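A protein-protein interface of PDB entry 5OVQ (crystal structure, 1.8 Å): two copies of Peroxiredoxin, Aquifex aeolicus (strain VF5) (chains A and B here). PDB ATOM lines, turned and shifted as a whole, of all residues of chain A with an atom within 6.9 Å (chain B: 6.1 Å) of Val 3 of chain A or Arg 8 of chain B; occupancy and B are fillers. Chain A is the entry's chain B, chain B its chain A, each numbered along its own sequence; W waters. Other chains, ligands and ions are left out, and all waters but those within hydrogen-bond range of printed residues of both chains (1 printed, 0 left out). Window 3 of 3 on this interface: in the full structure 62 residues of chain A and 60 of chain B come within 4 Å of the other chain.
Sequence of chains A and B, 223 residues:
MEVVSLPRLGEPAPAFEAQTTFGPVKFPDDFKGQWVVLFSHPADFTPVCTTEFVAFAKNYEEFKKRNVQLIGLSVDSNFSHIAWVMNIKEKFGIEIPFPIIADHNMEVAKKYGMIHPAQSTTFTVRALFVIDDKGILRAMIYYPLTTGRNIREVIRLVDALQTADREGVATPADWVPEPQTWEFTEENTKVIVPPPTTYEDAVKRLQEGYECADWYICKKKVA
Printed residues of chain A within 4 Å of Ser 5 of chain B: Val 4 (3.0 Å) and Leu 6 (3.8 Å). Of the printed residues of chain B, Val 4 of chain A touches Ser 5, Leu 6 and Arg 8. Of the printed residues of chain A, Gly 10 of chain B touches Ala 118. Of the printed residues of chain B, Gln 119 of chain A touches Leu 9. Printed residues of chain A within 4 Å of Pro 7 of chain B: His 116. Lys 111 of chain A touches none of the printed residues of chain B. The nearest residue of chain A that does not touch Arg 8 of chain B is Pro 117 of chain A (4.7 Å). The nearest printed residue of chain B that does not touch Gly 113 of chain A is Met 140 of chain B (6.3 Å).
OG of Ser 5 of chain B is in hydrogen-bond range of O of Val 4 of chain A. The backbone NH (N) of Leu 6 of chain B lies within hydrogen-bond range of the backbone carbonyl oxygen (O) of Val 4 of chain A (2.9 Å). N of Leu 9 of chain B lies within hydrogen-bond range of ND1 of His 116 of chain A. The guanidinium group (NH2) of Arg 8 of chain B sits close to the backbone NH (N) of Val 4 of chain A, at 3.0 Å.
Water W1 lies within hydrogen-bond range of the side-chain carboxylate of Glu 11 of chain B (2.8 Å), the backbone carbonyl oxygen of Leu 9 of chain B (2.8 Å) and the backbone NH of Ala 118 of chain A (2.9 Å).
OG of Ser 5 of chain B lies within hydrogen-bond range of NH1 of Arg 8 of chain B (3.3 Å). NH1 of Arg 8 of chain B sits at hydrogen-bond distance from O of Leu 6 of chain B. The backbone NH (N) of Gly 10 of chain B sits at hydrogen-bond distance from the backbone carbonyl oxygen (O) of Leu 137 of chain B, at 2.7 Å. O of Glu 11 of chain B sits at hydrogen-bond distance from N of Leu 137 of chain B, at 2.9 Å. The backbone carbonyl oxygen of Gly 113 of chain A lies within hydrogen-bond range of a ring nitrogen (NE2) of His 116 of chain A, at 2.7 Å.
Printed residues of chain B that touch a printed residue of chain A: Ser 5, Leu 6, Pro 7, Arg 8, Leu 9, Gly 10, Glu 11 and Met 140. Hydrophobic or aromatic side chains of chain B that line the printed part of chain A: Leu 6, Leu 9 and Met 140. Hydrophobic or aromatic side chains of chain A within 4 Å of the printed part of chain B: Val 4, Leu 6, His 116 and Ala 118. Along chain A the printed residues that touch a printed residue of chain B span positions 3 to 119. Among the printed residues, no Asp or Glu carboxylate lies within 4 Å of a Lys or Arg side-chain nitrogen of the other chain.
Ser 5 of chain A touches Leu 6 of chain B, and with the chains exchanged Leu 6 of chain A touches Ser 5 of chain B. Leu 6 of chain A touches its own counterpart, Leu 6 of chain B. Of the 17 pairs that touch across the chains among the printed residues, 3 have their exchanged pair printed and touching as well.
Arg 8 of chain B touches Val 3 of chain A. O of Ser 5 of chain B touches CB of Leu 6 of chain A, at 3.8 Å. CD1 of Leu 6 of chain A touches CD1 of Leu 6 of chain B, at 3.3 Å. O of Gly 113 of chain A touches CD2 of Leu 6 of chain B, 3.3 Å away. His 116 of chain A touches Leu 6 of chain B (NE2 to CD2, 3.5 Å). His 116 of chain A touches Arg 8 of chain B (ND1 to CA, 3.7 Å). CE1 of His 116 of chain A touches CE of Met 140 of chain B (3.6 Å). Leu 9 of chain B touches Ala 118 of chain A (O to CB, 3.6 Å). Ala 118 of chain A touches Gly 10 of chain B (CB to O, 3.5 Å). Ala 118 of chain A touches Glu 11 of chain B.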
ATOM      1  N   VAL A   3      -9.138  29.137  -8.624  1.00  0.00           N
ATOM      2  CA  VAL A   3      -9.177  28.399  -7.363  1.00  0.00           C
ATOM      3  C   VAL A   3      -8.679  29.282  -6.216  1.00  0.00           C
ATOM      4  O   VAL A   3      -7.662  29.973  -6.358  1.00  0.00           O
ATOM      5  CB  VAL A   3      -8.349  27.104  -7.449  1.00  0.00           C
ATOM      6  CG1 VAL A   3      -8.328  26.397  -6.103  1.00  0.00           C
ATOM      7  CG2 VAL A   3      -8.894  26.193  -8.524  1.00  0.00           C
ATOM      8  N   VAL A   4      -9.416  29.310  -5.103  1.00  0.00           N
ATOM      9  CA  VAL A   4     -10.751  28.719  -5.018  1.00  0.00           C
ATOM     10  C   VAL A   4     -11.712  29.736  -5.600  1.00  0.00           C
ATOM     11  O   VAL A   4     -12.062  30.720  -4.944  1.00  0.00           O
ATOM     12  CB  VAL A   4     -11.134  28.335  -3.563  1.00  0.00           C
ATOM     13  CG1 VAL A   4     -12.605  27.940  -3.466  1.00  0.00           C
ATOM     14  CG2 VAL A   4     -10.241  27.208  -3.051  1.00  0.00           C
ATOM     15  N   SER A   5     -12.095  29.540  -6.854  1.00  0.00           N
ATOM     16  CA  SER A   5     -12.910  30.547  -7.502  1.00  0.00           C
ATOM     17  C   SER A   5     -14.366  30.319  -7.149  1.00  0.00           C
ATOM     18  O   SER A   5     -14.803  29.197  -6.881  1.00  0.00           O
ATOM     19  CB  SER A   5     -12.715  30.536  -9.018  1.00  0.00           C
ATOM     20  OG  SER A   5     -13.116  31.778  -9.582  1.00  0.00           O
ATOM     21  N   LEU A   6     -15.106  31.407  -7.086  1.00  0.00           N
ATOM     22  CA  LEU A   6     -16.522  31.329  -6.811  1.00  0.00           C
ATOM     23  C   LEU A   6     -17.268  31.183  -8.125  1.00  0.00           C
ATOM     24  O   LEU A   6     -17.068  32.009  -9.025  1.00  0.00           O
ATOM     25  CB  LEU A   6     -16.991  32.568  -6.066  1.00  0.00           C
ATOM     26  CG  LEU A   6     -18.467  32.573  -5.686  1.00  0.00           C
ATOM     27  CD1 LEU A   6     -18.810  31.313  -4.935  1.00  0.00           C
ATOM     28  CD2 LEU A   6     -18.749  33.770  -4.815  1.00  0.00           C
ATOM     29  N   LYS A 110     -12.922  21.566  -8.377  1.00  0.00           N
ATOM     30  CA  LYS A 110     -12.223  22.846  -8.438  1.00  0.00           C
ATOM     31  C   LYS A 110     -12.995  23.875  -9.261  1.00  0.00           C
ATOM     32  O   LYS A 110     -12.955  25.069  -8.947  1.00  0.00           O
ATOM     33  CB  LYS A 110     -10.807  22.643  -8.976  1.00  0.00           C
ATOM     34  CG  LYS A 110      -9.890  21.968  -7.963  1.00  0.00           C
ATOM     35  CD  LYS A 110      -8.540  21.609  -8.567  1.00  0.00           C
ATOM     36  CE  LYS A 110      -7.634  20.971  -7.526  1.00  0.00           C
ATOM     37  NZ  LYS A 110      -6.600  20.091  -8.152  1.00  0.00           N
ATOM     38  N   LYS A 111     -13.672  23.441 -10.335  1.00  0.00           N
ATOM     39  CA  LYS A 111     -14.485  24.350 -11.136  1.00  0.00           C
ATOM     40  C   LYS A 111     -15.616  24.967 -10.324  1.00  0.00           C
ATOM     41  O   LYS A 111     -16.110  26.049 -10.667  1.00  0.00           O
ATOM     42  CB  LYS A 111     -15.080  23.626 -12.344  1.00  0.00           C
ATOM     43  CG  LYS A 111     -14.089  23.239 -13.421  1.00  0.00           C
ATOM     44  CD  LYS A 111     -14.773  22.486 -14.557  1.00  0.00           C
ATOM     45  CE  LYS A 111     -13.777  22.239 -15.706  1.00  0.00           C
ATOM     46  NZ  LYS A 111     -14.338  21.361 -16.772  1.00  0.00           N
ATOM     47  N   GLY A 113     -15.527  25.399  -6.889  1.00  0.00           N
ATOM     48  CA  GLY A 113     -15.058  25.879  -5.598  1.00  0.00           C
ATOM     49  C   GLY A 113     -15.385  24.954  -4.453  1.00  0.00           C
ATOM     50  O   GLY A 113     -15.573  25.410  -3.315  1.00  0.00           O
ATOM     51  N   ILE A 115     -13.462  22.546  -3.152  1.00  0.00           N
ATOM     52  CA  ILE A 115     -12.325  22.145  -2.334  1.00  0.00           C
ATOM     53  C   ILE A 115     -11.904  23.328  -1.476  1.00  0.00           C
ATOM     54  O   ILE A 115     -11.453  24.362  -1.998  1.00  0.00           O
ATOM     55  CB  ILE A 115     -11.150  21.657  -3.196  1.00  0.00           C
ATOM     56  CG1 ILE A 115     -11.624  20.595  -4.185  1.00  0.00           C
ATOM     57  CG2 ILE A 115     -10.065  21.100  -2.292  1.00  0.00           C
ATOM     58  CD1 ILE A 115     -12.171  19.348  -3.512  1.00  0.00           C
ATOM     59  N   HIS A 116     -12.029  23.163  -0.162  1.00  0.00           N
ATOM     60  CA  HIS A 116     -11.631  24.168   0.823  1.00  0.00           C
ATOM     61  C   HIS A 116     -10.547  23.570   1.698  1.00  0.00           C
ATOM     62  O   HIS A 116     -10.830  22.735   2.575  1.00  0.00           O
ATOM     63  CB  HIS A 116     -12.839  24.641   1.642  1.00  0.00           C
ATOM     64  CG  HIS A 116     -13.822  25.390   0.804  1.00  0.00           C
ATOM     65  ND1 HIS A 116     -14.069  26.741   0.967  1.00  0.00           N
ATOM     66  CD2 HIS A 116     -14.529  25.007  -0.289  1.00  0.00           C
ATOM     67  CE1 HIS A 116     -14.918  27.143   0.039  1.00  0.00           C
ATOM     68  NE2 HIS A 116     -15.214  26.115  -0.734  1.00  0.00           N
ATOM     69  N   PRO A 117      -9.288  23.936   1.465  1.00  0.00           N
ATOM     70  CA  PRO A 117      -8.172  23.161   2.034  1.00  0.00           C
ATOM     71  C   PRO A 117      -8.166  23.081   3.548  1.00  0.00           C
ATOM     72  O   PRO A 117      -7.735  22.057   4.095  1.00  0.00           O
ATOM     73  CB  PRO A 117      -6.935  23.904   1.504  1.00  0.00           C
ATOM     74  CG  PRO A 117      -7.402  24.595   0.264  1.00  0.00           C
ATOM     75  CD  PRO A 117      -8.838  24.992   0.536  1.00  0.00           C
ATOM     76  N   ALA A 118      -8.628  24.118   4.256  1.00  0.00           N
ATOM     77  CA  ALA A 118      -8.692  24.013   5.709  1.00  0.00           C
ATOM     78  C   ALA A 118      -9.754  23.020   6.154  1.00  0.00           C
ATOM     79  O   ALA A 118      -9.695  22.536   7.285  1.00  0.00           O
ATOM     80  CB  ALA A 118      -8.966  25.372   6.349  1.00  0.00           C
ATOM     81  N   GLN A 119     -10.738  22.733   5.299  1.00  0.00           N
ATOM     82  CA  GLN A 119     -11.675  21.640   5.559  1.00  0.00           C
ATOM     83  C   GLN A 119     -11.065  20.292   5.187  1.00  0.00           C
ATOM     84  O   GLN A 119     -11.003  19.365   6.007  1.00  0.00           O
ATOM     85  CB  GLN A 119     -12.964  21.883   4.767  1.00  0.00           C
ATOM     86  CG  GLN A 119     -13.866  22.945   5.381  1.00  0.00           C
ATOM     87  CD  GLN A 119     -14.847  22.314   6.359  1.00  0.00           C
ATOM     88  OE1 GLN A 119     -15.813  21.689   5.937  1.00  0.00           O
ATOM     89  NE2 GLN A 119     -14.563  22.406   7.649  1.00  0.00           N
ATOM     90  N   SER B   5     -13.150  36.001  -5.523  1.00  0.00           N
ATOM     91  CA  SER B   5     -12.758  34.662  -5.166  1.00  0.00           C
ATOM     92  C   SER B   5     -13.802  34.097  -4.234  1.00  0.00           C
ATOM     93  O   SER B   5     -14.745  34.780  -3.873  1.00  0.00           O
ATOM     94  CB  SER B   5     -11.375  34.641  -4.482  1.00  0.00           C
ATOM     95  OG  SER B   5     -10.736  33.369  -4.526  1.00  0.00           O
ATOM     96  N   LEU B   6     -13.644  32.837  -3.844  1.00  0.00           N
ATOM     97  CA  LEU B   6     -14.556  32.228  -2.890  1.00  0.00           C
ATOM     98  C   LEU B   6     -13.943  32.309  -1.508  1.00  0.00           C
ATOM     99  O   LEU B   6     -12.783  31.896  -1.343  1.00  0.00           O
ATOM    100  CB  LEU B   6     -14.847  30.778  -3.266  1.00  0.00           C
ATOM    101  CG  LEU B   6     -15.791  30.006  -2.352  1.00  0.00           C
ATOM    102  CD1 LEU B   6     -17.092  30.740  -2.128  1.00  0.00           C
ATOM    103  CD2 LEU B   6     -16.090  28.652  -2.957  1.00  0.00           C
ATOM    104  N   PRO B   7     -14.615  32.887  -0.515  1.00  0.00           N
ATOM    105  CA  PRO B   7     -14.089  32.808   0.849  1.00  0.00           C
ATOM    106  C   PRO B   7     -13.873  31.349   1.223  1.00  0.00           C
ATOM    107  O   PRO B   7     -14.599  30.455   0.780  1.00  0.00           O
ATOM    108  CB  PRO B   7     -15.182  33.465   1.699  1.00  0.00           C
ATOM    109  CG  PRO B   7     -15.939  34.306   0.734  1.00  0.00           C
ATOM    110  CD  PRO B   7     -15.927  33.557  -0.551  1.00  0.00           C
ATOM    111  N   ARG B   8     -12.874  31.116   2.057  1.00  0.00           N
ATOM    112  CA  ARG B   8     -12.392  29.764   2.320  1.00  0.00           C
ATOM    113  C   ARG B   8     -13.001  29.274   3.625  1.00  0.00           C
ATOM    114  O   ARG B   8     -12.765  29.870   4.679  1.00  0.00           O
ATOM    115  CB  ARG B   8     -10.870  29.750   2.437  1.00  0.00           C
ATOM    116  CG  ARG B   8     -10.082  30.172   1.204  1.00  0.00           C
ATOM    117  CD  ARG B   8     -10.376  29.372  -0.038  1.00  0.00           C
ATOM    118  NE  ARG B   8      -9.311  29.588  -1.018  1.00  0.00           N
ATOM    119  CZ  ARG B   8      -9.244  30.614  -1.864  1.00  0.00           C
ATOM    120  NH1 ARG B   8     -10.187  31.550  -1.875  1.00  0.00           N
ATOM    121  NH2 ARG B   8      -8.224  30.702  -2.706  1.00  0.00           N
ATOM    122  N   LEU B   9     -13.748  28.173   3.569  1.00  0.00           N
ATOM    123  CA  LEU B   9     -14.283  27.600   4.797  1.00  0.00           C
ATOM    124  C   LEU B   9     -13.151  27.100   5.679  1.00  0.00           C
ATOM    125  O   LEU B   9     -12.181  26.508   5.196  1.00  0.00           O
ATOM    126  CB  LEU B   9     -15.234  26.446   4.489  1.00  0.00           C
ATOM    127  CG  LEU B   9     -16.503  26.770   3.697  1.00  0.00           C
ATOM    128  CD1 LEU B   9     -17.339  25.505   3.527  1.00  0.00           C
ATOM    129  CD2 LEU B   9     -17.320  27.862   4.400  1.00  0.00           C
ATOM    130  N   GLY B  10     -13.272  27.353   6.976  1.00  0.00           N
ATOM    131  CA  GLY B  10     -12.282  26.904   7.924  1.00  0.00           C
ATOM    132  C   GLY B  10     -11.100  27.823   8.087  1.00  0.00           C
ATOM    133  O   GLY B  10     -10.206  27.519   8.887  1.00  0.00           O
ATOM    134  N   GLU B  11     -11.068  28.935   7.368  1.00  0.00           N
ATOM    135  CA  GLU B  11     -10.028  29.945   7.474  1.00  0.00           C
ATOM    136  C   GLU B  11     -10.594  31.220   8.088  1.00  0.00           C
ATOM    137  O   GLU B  11     -11.814  31.389   8.158  1.00  0.00           O
ATOM    138  CB  GLU B  11      -9.440  30.225   6.084  1.00  0.00           C
ATOM    139  CG  GLU B  11      -8.830  28.945   5.496  1.00  0.00           C
ATOM    140  CD  GLU B  11      -8.101  29.144   4.176  1.00  0.00           C
ATOM    141  OE1 GLU B  11      -7.637  30.274   3.892  1.00  0.00           O
ATOM    142  OE2 GLU B  11      -8.010  28.162   3.406  1.00  0.00           O
ATOM    143  N   PRO B  12      -9.742  32.125   8.579  1.00  0.00           N
ATOM    144  CA  PRO B  12     -10.261  33.364   9.177  1.00  0.00           C
ATOM    145  C   PRO B  12     -11.124  34.134   8.187  1.00  0.00           C
ATOM    146  O   PRO B  12     -10.815  34.223   7.001  1.00  0.00           O
ATOM    147  CB  PRO B  12      -8.993  34.137   9.549  1.00  0.00           C
ATOM    148  CG  PRO B  12      -7.978  33.065   9.805  1.00  0.00           C
ATOM    149  CD  PRO B  12      -8.294  31.961   8.817  1.00  0.00           C
ATOM    150  N   PRO B  14     -12.444  37.012   6.020  1.00  0.00           N
ATOM    151  CA  PRO B  14     -11.712  38.175   5.484  1.00  0.00           C
ATOM    152  C   PRO B  14     -11.911  39.423   6.336  1.00  0.00           C
ATOM    153  O   PRO B  14     -13.035  39.764   6.713  1.00  0.00           O
ATOM    154  CB  PRO B  14     -12.304  38.341   4.083  1.00  0.00           C
ATOM    155  CG  PRO B  14     -12.715  36.955   3.699  1.00  0.00           C
ATOM    156  CD  PRO B  14     -13.201  36.300   4.977  1.00  0.00           C
ATOM    157  N   LEU B 137     -14.517  31.293   9.305  1.00  0.00           N
ATOM    158  CA  LEU B 137     -15.669  31.092   8.428  1.00  0.00           C
ATOM    159  C   LEU B 137     -16.102  29.621   8.431  1.00  0.00           C
ATOM    160  O   LEU B 137     -15.294  28.727   8.165  1.00  0.00           O
ATOM    161  CB  LEU B 137     -15.335  31.553   7.014  1.00  0.00           C
ATOM    162  CG  LEU B 137     -16.458  31.333   6.009  1.00  0.00           C
ATOM    163  CD1 LEU B 137     -17.719  32.125   6.415  1.00  0.00           C
ATOM    164  CD2 LEU B 137     -15.970  31.714   4.619  1.00  0.00           C
ATOM    165  N   MET B 140     -21.529  29.065   4.321  1.00  0.00           N
ATOM    166  CA  MET B 140     -21.961  30.239   3.589  1.00  0.00           C
ATOM    167  C   MET B 140     -23.003  29.833   2.563  1.00  0.00           C
ATOM    168  O   MET B 140     -23.069  28.676   2.151  1.00  0.00           O
ATOM    169  CB  MET B 140     -20.764  30.929   2.911  1.00  0.00           C
ATOM    170  CG  MET B 140     -20.117  30.159   1.772  1.00  0.00           C
ATOM    171  SD  MET B 140     -18.481  30.851   1.381  1.00  0.00           S
ATOM    172  CE  MET B 140     -17.529  29.355   1.158  1.00  0.00           C
HETATM  173  O   HOH W   1     -10.177  26.381   3.201  1.00  0.00           O
